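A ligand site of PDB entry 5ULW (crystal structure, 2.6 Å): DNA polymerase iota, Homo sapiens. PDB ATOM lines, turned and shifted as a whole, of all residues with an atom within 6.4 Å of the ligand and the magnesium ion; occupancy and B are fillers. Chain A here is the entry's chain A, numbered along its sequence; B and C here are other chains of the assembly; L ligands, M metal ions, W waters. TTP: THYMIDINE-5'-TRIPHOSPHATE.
OD1 of Asp 34 is bound to the magnesium ion (2.0 Å).
The side-chain carboxylate (OD2) of Asp 126 binds the magnesium ion (2.1 Å).
The magnesium ion is bound by O of Leu 35 (2.1 Å).
The magnesium ion is bound by O1B of the ligand (2.3 Å).
O1A of the ligand binds the magnesium ion, at 2.4 Å.
O3G of the ligand is bound to the magnesium ion (2.5 Å).
The magnesium ion has six donor atoms within binding distance.
The guanidinium group (NE) of Arg 71 lies within hydrogen-bond range of the backbone carbonyl oxygen (O) of Cys 66.
N2 of DG 5 of chain B lies close to O2 of DOC 7 of chain C (2.6 Å).
OH of Tyr 68 lies within hydrogen-bond range of NH1 of Arg 71, 3.3 Å away.
The backbone NH (N) of Leu 78 lies within hydrogen-bond range of the backbone carbonyl oxygen (O) of Val 64 (3.3 Å).
Water W1 lies within hydrogen-bond range of an oxygen (O2) of the ligand (2.5 Å), the side-chain hydroxyl of Tyr 39 (2.6 Å), N3 of DG 5 of chain B (2.7 Å) and the side-chain amide nitrogen of Gln 59 (3.5 Å).
Water W4 lies within hydrogen-bond range of the side-chain carboxylate of Asp 36 (2.4 Å), the side-chain hydroxyl of Tyr 68 (2.6 Å) and an oxygen (O1G) of the ligand (3.3 Å).
The backbone NH (N) of Cys 37 lies within hydrogen-bond range of an oxygen (O1G) of the ligand, 2.8 Å away.
The side-chain hydroxyl (OH) of Tyr 68 lies within hydrogen-bond range of an oxygen (O1G) of the ligand (2.5 Å).
O2G of the ligand lies within salt-bridge range of NZ of Lys 214 (3.0 Å).
N of Phe 38 is in hydrogen-bond range of O2B of the ligand, 3.3 Å away.
N3 of the ligand is in hydrogen-bond range of N7 of MA7 4 of chain B (3.2 Å).
O2G of the ligand lies within salt-bridge range of NZ of Lys 77, 2.9 Å away.
The side-chain hydroxyl of Thr 65 sits at hydrogen-bond distance from an oxygen (O2B) of the ligand.
N1 of DG 5 of chain B is in hydrogen-bond range of a nitrogen (N3) of the ligand, 3.4 Å away.
NH1 of Arg 71 is in salt-bridge range of O2G of the ligand.
The backbone NH of Tyr 39 sits at hydrogen-bond distance from an oxygen (O3') of the ligand.
Merely in contact with the ligand: Val 64 (3.1 Å), DOC 7 of chain C (3.5 Å), Asp 36 (3.6 Å) and Glu 127 (3.98 Å).
Within 4 Å of the ligand: Asp 34, Leu 35, Asp 36, Cys 37, Phe 38, Tyr 39, Val 64, Thr 65, Tyr 68, Arg 71, Lys 77, Asp 126, Glu 127, Lys 214, MA7 4 of chain B, DG 5 of chain B and DOC 7 of chain C.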
ATOM      1  N   ASP A  34      16.431 -33.151  -0.982  1.00  0.00           N
ATOM      2  CA  ASP A  34      16.819 -32.149  -1.972  1.00  0.00           C
ATOM      3  C   ASP A  34      18.306 -31.852  -1.815  1.00  0.00           C
ATOM      4  O   ASP A  34      18.724 -31.305  -0.792  1.00  0.00           O
ATOM      5  CB  ASP A  34      16.005 -30.861  -1.801  1.00  0.00           C
ATOM      6  CG  ASP A  34      16.406 -29.776  -2.785  1.00  0.00           C
ATOM      7  OD1 ASP A  34      17.471 -29.898  -3.431  1.00  0.00           O
ATOM      8  OD2 ASP A  34      15.641 -28.787  -2.906  1.00  0.00           O
ATOM      9  N   LEU A  35      19.097 -32.207  -2.821  1.00  0.00           N
ATOM     10  CA  LEU A  35      20.549 -32.174  -2.672  1.00  0.00           C
ATOM     11  C   LEU A  35      21.108 -30.760  -2.778  1.00  0.00           C
ATOM     12  O   LEU A  35      20.524 -29.874  -3.425  1.00  0.00           O
ATOM     13  CB  LEU A  35      21.206 -33.088  -3.699  1.00  0.00           C
ATOM     14  CG  LEU A  35      20.704 -34.534  -3.524  1.00  0.00           C
ATOM     15  CD1 LEU A  35      21.588 -35.542  -4.216  1.00  0.00           C
ATOM     16  CD2 LEU A  35      20.618 -34.849  -2.067  1.00  0.00           C
ATOM     17  N   ASP A  36      22.240 -30.538  -2.102  1.00  0.00           N
ATOM     18  CA  ASP A  36      22.990 -29.296  -2.210  1.00  0.00           C
ATOM     19  C   ASP A  36      23.614 -29.099  -3.603  1.00  0.00           C
ATOM     20  O   ASP A  36      24.266 -30.000  -4.143  1.00  0.00           O
ATOM     21  CB  ASP A  36      24.098 -29.266  -1.152  1.00  0.00           C
ATOM     22  CG  ASP A  36      23.575 -29.525   0.263  1.00  0.00           C
ATOM     23  OD1 ASP A  36      22.431 -29.116   0.563  1.00  0.00           O
ATOM     24  OD2 ASP A  36      24.323 -30.138   1.070  1.00  0.00           O
ATOM     25  N   CYS A  37      23.418 -27.894  -4.168  1.00  0.00           N
ATOM     26  CA  CYS A  37      24.083 -27.454  -5.390  1.00  0.00           C
ATOM     27  C   CYS A  37      24.523 -28.631  -6.269  1.00  0.00           C
ATOM     28  O   CYS A  37      25.713 -28.843  -6.521  1.00  0.00           O
ATOM     29  CB  CYS A  37      25.270 -26.571  -5.019  1.00  0.00           C
ATOM     30  SG  CYS A  37      26.460 -27.315  -3.854  1.00  0.00           S
ATOM     31  N   PHE A  38      23.543 -29.387  -6.756  1.00  0.00           N
ATOM     32  CA  PHE A  38      23.780 -30.767  -7.203  1.00  0.00           C
ATOM     33  C   PHE A  38      24.868 -30.860  -8.266  1.00  0.00           C
ATOM     34  O   PHE A  38      25.798 -31.673  -8.160  1.00  0.00           O
ATOM     35  CB  PHE A  38      22.473 -31.375  -7.709  1.00  0.00           C
ATOM     36  CG  PHE A  38      22.620 -32.768  -8.179  1.00  0.00           C
ATOM     37  CD1 PHE A  38      23.190 -33.731  -7.353  1.00  0.00           C
ATOM     38  CD2 PHE A  38      22.238 -33.121  -9.456  1.00  0.00           C
ATOM     39  CE1 PHE A  38      23.334 -35.044  -7.788  1.00  0.00           C
ATOM     40  CE2 PHE A  38      22.385 -34.424  -9.893  1.00  0.00           C
ATOM     41  CZ  PHE A  38      22.934 -35.381  -9.060  1.00  0.00           C
ATOM     42  N   TYR A  39      24.761 -30.078  -9.337  1.00  0.00           N
ATOM     43  CA  TYR A  39      25.780 -30.180 -10.374  1.00  0.00           C
ATOM     44  C   TYR A  39      27.143 -29.794  -9.807  1.00  0.00           C
ATOM     45  O   TYR A  39      28.136 -30.517  -9.972  1.00  0.00           O
ATOM     46  CB  TYR A  39      25.433 -29.292 -11.581  1.00  0.00           C
ATOM     47  CG  TYR A  39      24.266 -29.734 -12.460  1.00  0.00           C
ATOM     48  CD1 TYR A  39      23.474 -30.863 -12.149  1.00  0.00           C
ATOM     49  CD2 TYR A  39      23.957 -29.013 -13.616  1.00  0.00           C
ATOM     50  CE1 TYR A  39      22.422 -31.248 -12.970  1.00  0.00           C
ATOM     51  CE2 TYR A  39      22.921 -29.392 -14.438  1.00  0.00           C
ATOM     52  CZ  TYR A  39      22.157 -30.493 -14.111  1.00  0.00           C
ATOM     53  OH  TYR A  39      21.128 -30.817 -14.965  1.00  0.00           O
ATOM     54  N   ALA A  40      27.192 -28.658  -9.121  1.00  0.00           N
ATOM     55  CA  ALA A  40      28.430 -28.265  -8.458  1.00  0.00           C
ATOM     56  C   ALA A  40      28.961 -29.387  -7.586  1.00  0.00           C
ATOM     57  O   ALA A  40      30.155 -29.718  -7.636  1.00  0.00           O
ATOM     58  CB  ALA A  40      28.197 -26.992  -7.638  1.00  0.00           C
ATOM     59  N   GLN A  59      26.666 -23.404 -18.463  1.00  0.00           N
ATOM     60  CA  GLN A  59      26.037 -23.961 -19.645  1.00  0.00           C
ATOM     61  C   GLN A  59      25.802 -22.797 -20.583  1.00  0.00           C
ATOM     62  O   GLN A  59      24.988 -21.923 -20.278  1.00  0.00           O
ATOM     63  CB  GLN A  59      24.708 -24.660 -19.299  1.00  0.00           C
ATOM     64  CG  GLN A  59      24.833 -25.958 -18.484  1.00  0.00           C
ATOM     65  CD  GLN A  59      23.466 -26.540 -18.123  1.00  0.00           C
ATOM     66  OE1 GLN A  59      22.495 -25.813 -17.966  1.00  0.00           O
ATOM     67  NE2 GLN A  59      23.395 -27.861 -18.004  1.00  0.00           N
ATOM     68  N   VAL A  64      24.342 -22.037 -14.094  1.00  0.00           N
ATOM     69  CA  VAL A  64      23.082 -22.687 -13.730  1.00  0.00           C
ATOM     70  C   VAL A  64      23.011 -22.902 -12.227  1.00  0.00           C
ATOM     71  O   VAL A  64      21.980 -22.666 -11.595  1.00  0.00           O
ATOM     72  CB  VAL A  64      22.896 -24.005 -14.500  1.00  0.00           C
ATOM     73  CG1 VAL A  64      21.581 -24.642 -14.137  1.00  0.00           C
ATOM     74  CG2 VAL A  64      22.945 -23.761 -15.994  1.00  0.00           C
ATOM     75  N   THR A  65      24.113 -23.326 -11.623  1.00  0.00           N
ATOM     76  CA  THR A  65      24.188 -23.484 -10.178  1.00  0.00           C
ATOM     77  C   THR A  65      25.622 -23.203  -9.744  1.00  0.00           C
ATOM     78  O   THR A  65      26.558 -23.271 -10.541  1.00  0.00           O
ATOM     79  CB  THR A  65      23.750 -24.884  -9.740  1.00  0.00           C
ATOM     80  OG1 THR A  65      23.800 -24.965  -8.308  1.00  0.00           O
ATOM     81  CG2 THR A  65      24.694 -25.935 -10.310  1.00  0.00           C
ATOM     82  N   CYS A  66      25.793 -22.941  -8.445  1.00  0.00           N
ATOM     83  CA  CYS A  66      27.108 -22.717  -7.853  1.00  0.00           C
ATOM     84  C   CYS A  66      27.130 -23.312  -6.462  1.00  0.00           C
ATOM     85  O   CYS A  66      26.073 -23.522  -5.840  1.00  0.00           O
ATOM     86  CB  CYS A  66      27.477 -21.233  -7.781  1.00  0.00           C
ATOM     87  SG  CYS A  66      26.226 -20.237  -7.019  1.00  0.00           S
ATOM     88  N   TYR A  68      28.189 -23.537  -2.340  1.00  0.00           N
ATOM     89  CA  TYR A  68      27.800 -22.565  -1.323  1.00  0.00           C
ATOM     90  C   TYR A  68      28.926 -21.607  -1.015  1.00  0.00           C
ATOM     91  O   TYR A  68      28.670 -20.437  -0.701  1.00  0.00           O
ATOM     92  CB  TYR A  68      27.285 -23.286  -0.067  1.00  0.00           C
ATOM     93  CG  TYR A  68      25.867 -23.730  -0.298  1.00  0.00           C
ATOM     94  CD1 TYR A  68      25.588 -24.834  -1.106  1.00  0.00           C
ATOM     95  CD2 TYR A  68      24.798 -23.024   0.225  1.00  0.00           C
ATOM     96  CE1 TYR A  68      24.261 -25.230  -1.356  1.00  0.00           C
ATOM     97  CE2 TYR A  68      23.478 -23.418  -0.004  1.00  0.00           C
ATOM     98  CZ  TYR A  68      23.213 -24.523  -0.798  1.00  0.00           C
ATOM     99  OH  TYR A  68      21.912 -24.906  -1.058  1.00  0.00           O
ATOM    100  N   ARG A  71      28.041 -18.934  -3.195  1.00  0.00           N
ATOM    101  CA  ARG A  71      26.855 -18.150  -2.849  1.00  0.00           C
ATOM    102  C   ARG A  71      27.154 -17.183  -1.699  1.00  0.00           C
ATOM    103  O   ARG A  71      26.447 -16.174  -1.537  1.00  0.00           O
ATOM    104  CB  ARG A  71      25.685 -19.065  -2.502  1.00  0.00           C
ATOM    105  CG  ARG A  71      25.245 -19.981  -3.622  1.00  0.00           C
ATOM    106  CD  ARG A  71      24.039 -20.863  -3.252  1.00  0.00           C
ATOM    107  NE  ARG A  71      24.062 -22.100  -4.044  1.00  0.00           N
ATOM    108  CZ  ARG A  71      23.040 -22.944  -4.168  1.00  0.00           C
ATOM    109  NH1 ARG A  71      21.908 -22.708  -3.562  1.00  0.00           N
ATOM    110  NH2 ARG A  71      23.169 -24.041  -4.916  1.00  0.00           N
ATOM    111  N   LYS A  77      22.096 -18.712  -8.221  1.00  0.00           N
ATOM    112  CA  LYS A  77      21.741 -19.693  -9.244  1.00  0.00           C
ATOM    113  C   LYS A  77      21.144 -18.996 -10.452  1.00  0.00           C
ATOM    114  O   LYS A  77      20.263 -18.139 -10.322  1.00  0.00           O
ATOM    115  CB  LYS A  77      20.743 -20.724  -8.679  1.00  0.00           C
ATOM    116  CG  LYS A  77      21.381 -21.657  -7.666  1.00  0.00           C
ATOM    117  CD  LYS A  77      20.404 -22.593  -7.019  1.00  0.00           C
ATOM    118  CE  LYS A  77      19.196 -21.889  -6.470  1.00  0.00           C
ATOM    119  NZ  LYS A  77      18.354 -22.824  -5.647  1.00  0.00           N
ATOM    120  N   LEU A  78      21.644 -19.335 -11.633  1.00  0.00           N
ATOM    121  CA  LEU A  78      21.041 -18.909 -12.891  1.00  0.00           C
ATOM    122  C   LEU A  78      21.356 -17.471 -13.290  1.00  0.00           C
ATOM    123  O   LEU A  78      20.617 -16.878 -14.078  1.00  0.00           O
ATOM    124  CB  LEU A  78      19.526 -19.099 -12.857  1.00  0.00           C
ATOM    125  CG  LEU A  78      19.069 -20.557 -12.954  1.00  0.00           C
ATOM    126  CD1 LEU A  78      17.581 -20.710 -12.691  1.00  0.00           C
ATOM    127  CD2 LEU A  78      19.429 -21.070 -14.343  1.00  0.00           C
ATOM    128  N   LEU A  99      24.921 -33.764 -19.324  1.00  0.00           N
ATOM    129  CA  LEU A  99      24.279 -34.163 -18.081  1.00  0.00           C
ATOM    130  C   LEU A  99      24.586 -35.590 -17.708  1.00  0.00           C
ATOM    131  O   LEU A  99      24.005 -36.089 -16.743  1.00  0.00           O
ATOM    132  CB  LEU A  99      22.782 -33.985 -18.175  1.00  0.00           C
ATOM    133  CG  LEU A  99      22.285 -32.598 -18.557  1.00  0.00           C
ATOM    134  CD1 LEU A  99      20.757 -32.503 -18.469  1.00  0.00           C
ATOM    135  CD2 LEU A  99      22.928 -31.577 -17.664  1.00  0.00           C
ATOM    136  N   PHE A 125      16.374 -33.660 -11.219  1.00  0.00           N
ATOM    137  CA  PHE A 125      17.485 -34.590 -11.003  1.00  0.00           C
ATOM    138  C   PHE A 125      17.923 -34.720  -9.552  1.00  0.00           C
ATOM    139  O   PHE A 125      18.635 -35.672  -9.249  1.00  0.00           O
ATOM    140  CB  PHE A 125      18.730 -34.191 -11.817  1.00  0.00           C
ATOM    141  CG  PHE A 125      18.657 -34.542 -13.289  1.00  0.00           C
ATOM    142  CD1 PHE A 125      17.435 -34.743 -13.917  1.00  0.00           C
ATOM    143  CD2 PHE A 125      19.831 -34.648 -14.042  1.00  0.00           C
ATOM    144  CE1 PHE A 125      17.370 -35.051 -15.268  1.00  0.00           C
ATOM    145  CE2 PHE A 125      19.773 -34.956 -15.386  1.00  0.00           C
ATOM    146  CZ  PHE A 125      18.535 -35.164 -16.012  1.00  0.00           C
ATOM    147  N   ASP A 126      17.561 -33.798  -8.649  1.00  0.00           N
ATOM    148  CA  ASP A 126      18.085 -33.936  -7.299  1.00  0.00           C
ATOM    149  C   ASP A 126      17.031 -33.826  -6.212  1.00  0.00           C
ATOM    150  O   ASP A 126      17.373 -33.499  -5.066  1.00  0.00           O
ATOM    151  CB  ASP A 126      19.209 -32.929  -7.014  1.00  0.00           C
ATOM    152  CG  ASP A 126      18.681 -31.555  -6.688  1.00  0.00           C
ATOM    153  OD1 ASP A 126      17.646 -31.155  -7.274  1.00  0.00           O
ATOM    154  OD2 ASP A 126      19.316 -30.876  -5.846  1.00  0.00           O
ATOM    155  N   GLU A 127      15.754 -34.110  -6.520  1.00  0.00           N
ATOM    156  CA  GLU A 127      14.725 -34.140  -5.479  1.00  0.00           C
ATOM    157  C   GLU A 127      13.926 -35.447  -5.552  1.00  0.00           C
ATOM    158  O   GLU A 127      13.660 -35.970  -6.642  1.00  0.00           O
ATOM    159  CB  GLU A 127      13.763 -32.938  -5.563  1.00  0.00           C
ATOM    160  CG  GLU A 127      14.432 -31.588  -5.372  1.00  0.00           C
ATOM    161  CD  GLU A 127      13.448 -30.430  -5.605  1.00  0.00           C
ATOM    162  OE1 GLU A 127      12.234 -30.623  -5.363  1.00  0.00           O
ATOM    163  OE2 GLU A 127      13.880 -29.328  -6.024  1.00  0.00           O
ATOM    164  N   LYS A 214      19.484 -24.582   4.934  1.00  0.00           N
ATOM    165  CA  LYS A 214      20.420 -25.029   3.906  1.00  0.00           C
ATOM    166  C   LYS A 214      21.813 -24.505   4.195  1.00  0.00           C
ATOM    167  O   LYS A 214      21.978 -23.439   4.775  1.00  0.00           O
ATOM    168  CB  LYS A 214      19.948 -24.551   2.534  1.00  0.00           C
ATOM    169  CG  LYS A 214      18.689 -25.259   2.060  1.00  0.00           C
ATOM    170  CD  LYS A 214      17.996 -24.499   0.950  1.00  0.00           C
ATOM    171  CE  LYS A 214      18.938 -24.170  -0.173  1.00  0.00           C
ATOM    172  NZ  LYS A 214      18.174 -23.492  -1.257  1.00  0.00           N
ATOM    173  N   PRO A 215      22.839 -25.261   3.797  1.00  0.00           N
ATOM    174  CA  PRO A 215      22.730 -26.582   3.162  1.00  0.00           C
ATOM    175  C   PRO A 215      22.845 -27.731   4.136  1.00  0.00           C
ATOM    176  O   PRO A 215      23.091 -27.497   5.330  1.00  0.00           O
ATOM    177  CB  PRO A 215      23.916 -26.589   2.231  1.00  0.00           C
ATOM    178  CG  PRO A 215      24.959 -25.936   3.074  1.00  0.00           C
ATOM    179  CD  PRO A 215      24.229 -24.773   3.733  1.00  0.00           C
ATOM    180  C2  MA7 B   4      17.105 -21.566 -19.995  1.00  0.00           C
ATOM    181  C4  MA7 B   4      18.656 -23.179 -19.347  1.00  0.00           C
ATOM    182  C5  MA7 B   4      17.942 -23.408 -18.234  1.00  0.00           C
ATOM    183  C6  MA7 B   4      16.774 -22.712 -17.994  1.00  0.00           C
ATOM    184  C8  MA7 B   4      19.691 -24.752 -18.167  1.00  0.00           C
ATOM    185  P   MA7 B   4      20.656 -19.666 -23.576  1.00  0.00           P
ATOM    186  OP1 MA7 B   4      21.641 -19.704 -24.703  1.00  0.00           O
ATOM    187  OP2 MA7 B   4      19.233 -19.637 -24.133  1.00  0.00           O
ATOM    188  O5' MA7 B   4      20.802 -21.024 -22.671  1.00  0.00           O
ATOM    189  N9  MA7 B   4      19.732 -23.997 -19.302  1.00  0.00           N
ATOM    190  N3  MA7 B   4      18.253 -22.257 -20.228  1.00  0.00           N
ATOM    191  N1  MA7 B   4      16.359 -21.805 -18.865  1.00  0.00           N
ATOM    192  N6  MA7 B   4      16.087 -23.089 -16.747  1.00  0.00           N
ATOM    193  N7  MA7 B   4      18.575 -24.386 -17.515  1.00  0.00           N
ATOM    194  CN  MA7 B   4      15.145 -20.977 -18.814  1.00  0.00           C
ATOM    195  C2' MA7 B   4      20.336 -24.395 -21.792  1.00  0.00           C
ATOM    196  C5' MA7 B   4      22.087 -21.546 -22.623  1.00  0.00           C
ATOM    197  C4' MA7 B   4      22.100 -22.835 -21.908  1.00  0.00           C
ATOM    198  O4' MA7 B   4      21.282 -22.803 -20.438  1.00  0.00           O
ATOM    199  C1' MA7 B   4      20.803 -24.032 -20.303  1.00  0.00           C
ATOM    200  C3' MA7 B   4      21.572 -23.847 -22.604  1.00  0.00           C
ATOM    201  O3' MA7 B   4      22.607 -24.867 -22.571  1.00  0.00           O
ATOM    202  P    DG B   5      22.574 -26.081 -23.588  1.00  0.00           P
ATOM    203  OP1  DG B   5      23.962 -26.561 -23.838  1.00  0.00           O
ATOM    204  OP2  DG B   5      21.696 -25.611 -24.696  1.00  0.00           O
ATOM    205  O5'  DG B   5      21.834 -27.229 -22.764  1.00  0.00           O
ATOM    206  C5'  DG B   5      22.570 -28.036 -21.841  1.00  0.00           C
ATOM    207  C4'  DG B   5      21.659 -29.029 -21.192  1.00  0.00           C
ATOM    208  O4'  DG B   5      20.694 -28.318 -20.349  1.00  0.00           O
ATOM    209  C3'  DG B   5      20.808 -29.859 -22.166  1.00  0.00           C
ATOM    210  O3'  DG B   5      20.710 -31.176 -21.680  1.00  0.00           O
ATOM    211  C2'  DG B   5      19.463 -29.154 -22.103  1.00  0.00           C
ATOM    212  C1'  DG B   5      19.428 -28.857 -20.610  1.00  0.00           C
ATOM    213  N9   DG B   5      18.399 -27.902 -20.214  1.00  0.00           N
ATOM    214  C8   DG B   5      17.833 -26.919 -20.987  1.00  0.00           C
ATOM    215  N7   DG B   5      16.909 -26.240 -20.369  1.00  0.00           N
ATOM    216  C5   DG B   5      16.840 -26.829 -19.113  1.00  0.00           C
ATOM    217  C6   DG B   5      16.017 -26.509 -18.006  1.00  0.00           C
ATOM    218  O6   DG B   5      15.161 -25.613 -17.913  1.00  0.00           O
ATOM    219  N1   DG B   5      16.282 -27.325 -16.911  1.00  0.00           N
ATOM    220  C2   DG B   5      17.218 -28.337 -16.906  1.00  0.00           C
ATOM    221  N2   DG B   5      17.329 -29.033 -15.764  1.00  0.00           N
ATOM    222  N3   DG B   5      17.983 -28.649 -17.940  1.00  0.00           N
ATOM    223  C4   DG B   5      17.751 -27.845 -18.998  1.00  0.00           C
ATOM    224  N1  DOC C   7      13.988 -28.252 -12.402  1.00  0.00           N
ATOM    225  C2  DOC C   7      14.883 -28.247 -13.578  1.00  0.00           C
ATOM    226  N3  DOC C   7      14.665 -27.261 -14.656  1.00  0.00           N
ATOM    227  C4  DOC C   7      13.590 -26.307 -14.539  1.00  0.00           C
ATOM    228  C5  DOC C   7      12.707 -26.294 -13.359  1.00  0.00           C
ATOM    229  C6  DOC C   7      12.916 -27.286 -12.272  1.00  0.00           C
ATOM    230  O2  DOC C   7      15.763 -29.042 -13.662  1.00  0.00           O
ATOM    231  N4  DOC C   7      13.391 -25.363 -15.595  1.00  0.00           N
ATOM    232  C1' DOC C   7      14.225 -29.192 -11.384  1.00  0.00           C
ATOM    233  C2' DOC C   7      15.179 -28.733 -10.574  1.00  0.00           C
ATOM    234  C3' DOC C   7      14.427 -28.110  -9.382  1.00  0.00           C
ATOM    235  C4' DOC C   7      13.142 -29.066  -9.277  1.00  0.00           C
ATOM    236  O4' DOC C   7      12.847 -29.387 -10.497  1.00  0.00           O
ATOM    237  C5' DOC C   7      11.945 -28.340  -8.653  1.00  0.00           C
ATOM    238  O5' DOC C   7      11.813 -27.078  -9.223  1.00  0.00           O
ATOM    239  P   DOC C   7      10.470 -26.333  -8.679  1.00  0.00           P
ATOM    240  OP1 DOC C   7      10.681 -26.253  -7.188  1.00  0.00           O
ATOM    241  OP2 DOC C   7      10.295 -24.987  -9.357  1.00  0.00           O
HETATM  242  PA  TTP L   1      17.989 -27.253  -7.566  1.00  0.00           P
HETATM  243  O1A TTP L   1      17.693 -28.324  -6.545  1.00  0.00           O
HETATM  244  O2A TTP L   1      16.892 -26.229  -7.763  1.00  0.00           O
HETATM  245  O3A TTP L   1      19.267 -26.380  -7.188  1.00  0.00           O
HETATM  246  PB  TTP L   1      20.631 -26.927  -6.568  1.00  0.00           P
HETATM  247  O1B TTP L   1      20.589 -28.336  -6.002  1.00  0.00           O
HETATM  248  O2B TTP L   1      21.736 -26.730  -7.577  1.00  0.00           O
HETATM  249  O3B TTP L   1      20.748 -25.750  -5.481  1.00  0.00           O
HETATM  250  PG  TTP L   1      20.217 -25.852  -3.966  1.00  0.00           P
HETATM  251  O1G TTP L   1      21.427 -26.172  -3.126  1.00  0.00           O
HETATM  252  O2G TTP L   1      19.658 -24.485  -3.609  1.00  0.00           O
HETATM  253  O3G TTP L   1      19.146 -26.907  -3.783  1.00  0.00           O
HETATM  254  O5' TTP L   1      18.443 -27.860  -8.997  1.00  0.00           O
HETATM  255  C5' TTP L   1      19.103 -29.120  -9.111  1.00  0.00           C
HETATM  256  C4' TTP L   1      20.062 -29.124 -10.309  1.00  0.00           C
HETATM  257  O4' TTP L   1      19.353 -29.111 -11.566  1.00  0.00           O
HETATM  258  C3' TTP L   1      21.020 -27.916 -10.330  1.00  0.00           C
HETATM  259  O3' TTP L   1      22.303 -28.228  -9.789  1.00  0.00           O
HETATM  260  C2' TTP L   1      21.128 -27.512 -11.790  1.00  0.00           C
HETATM  261  C1' TTP L   1      19.958 -28.199 -12.479  1.00  0.00           C
HETATM  262  N1  TTP L   1      18.990 -27.169 -12.862  1.00  0.00           N
HETATM  263  C2  TTP L   1      19.066 -26.676 -14.172  1.00  0.00           C
HETATM  264  O2  TTP L   1      19.914 -27.139 -14.957  1.00  0.00           O
HETATM  265  N3  TTP L   1      18.222 -25.737 -14.598  1.00  0.00           N
HETATM  266  C4  TTP L   1      17.307 -25.214 -13.800  1.00  0.00           C
HETATM  267  O4  TTP L   1      16.532 -24.323 -14.226  1.00  0.00           O
HETATM  268  C5  TTP L   1      17.199 -25.684 -12.414  1.00  0.00           C
HETATM  269  C5M TTP L   1      16.146 -25.069 -11.529  1.00  0.00           C
HETATM  270  C6  TTP L   1      18.089 -26.677 -11.993  1.00  0.00           C
HETATM  271 MG    MG M   1      18.916 -29.209  -4.657  1.00  0.00          MG
HETATM  272  O   HOH W   1      20.376 -28.948 -16.640  1.00  0.00           O
HETATM  273  O   HOH W   2      16.600 -26.232  -3.596  1.00  0.00           O
HETATM  274  O   HOH W   3      19.007 -28.577  -1.222  1.00  0.00           O
HETATM  275  O   HOH W   4      21.068 -27.164   0.012  1.00  0.00           O
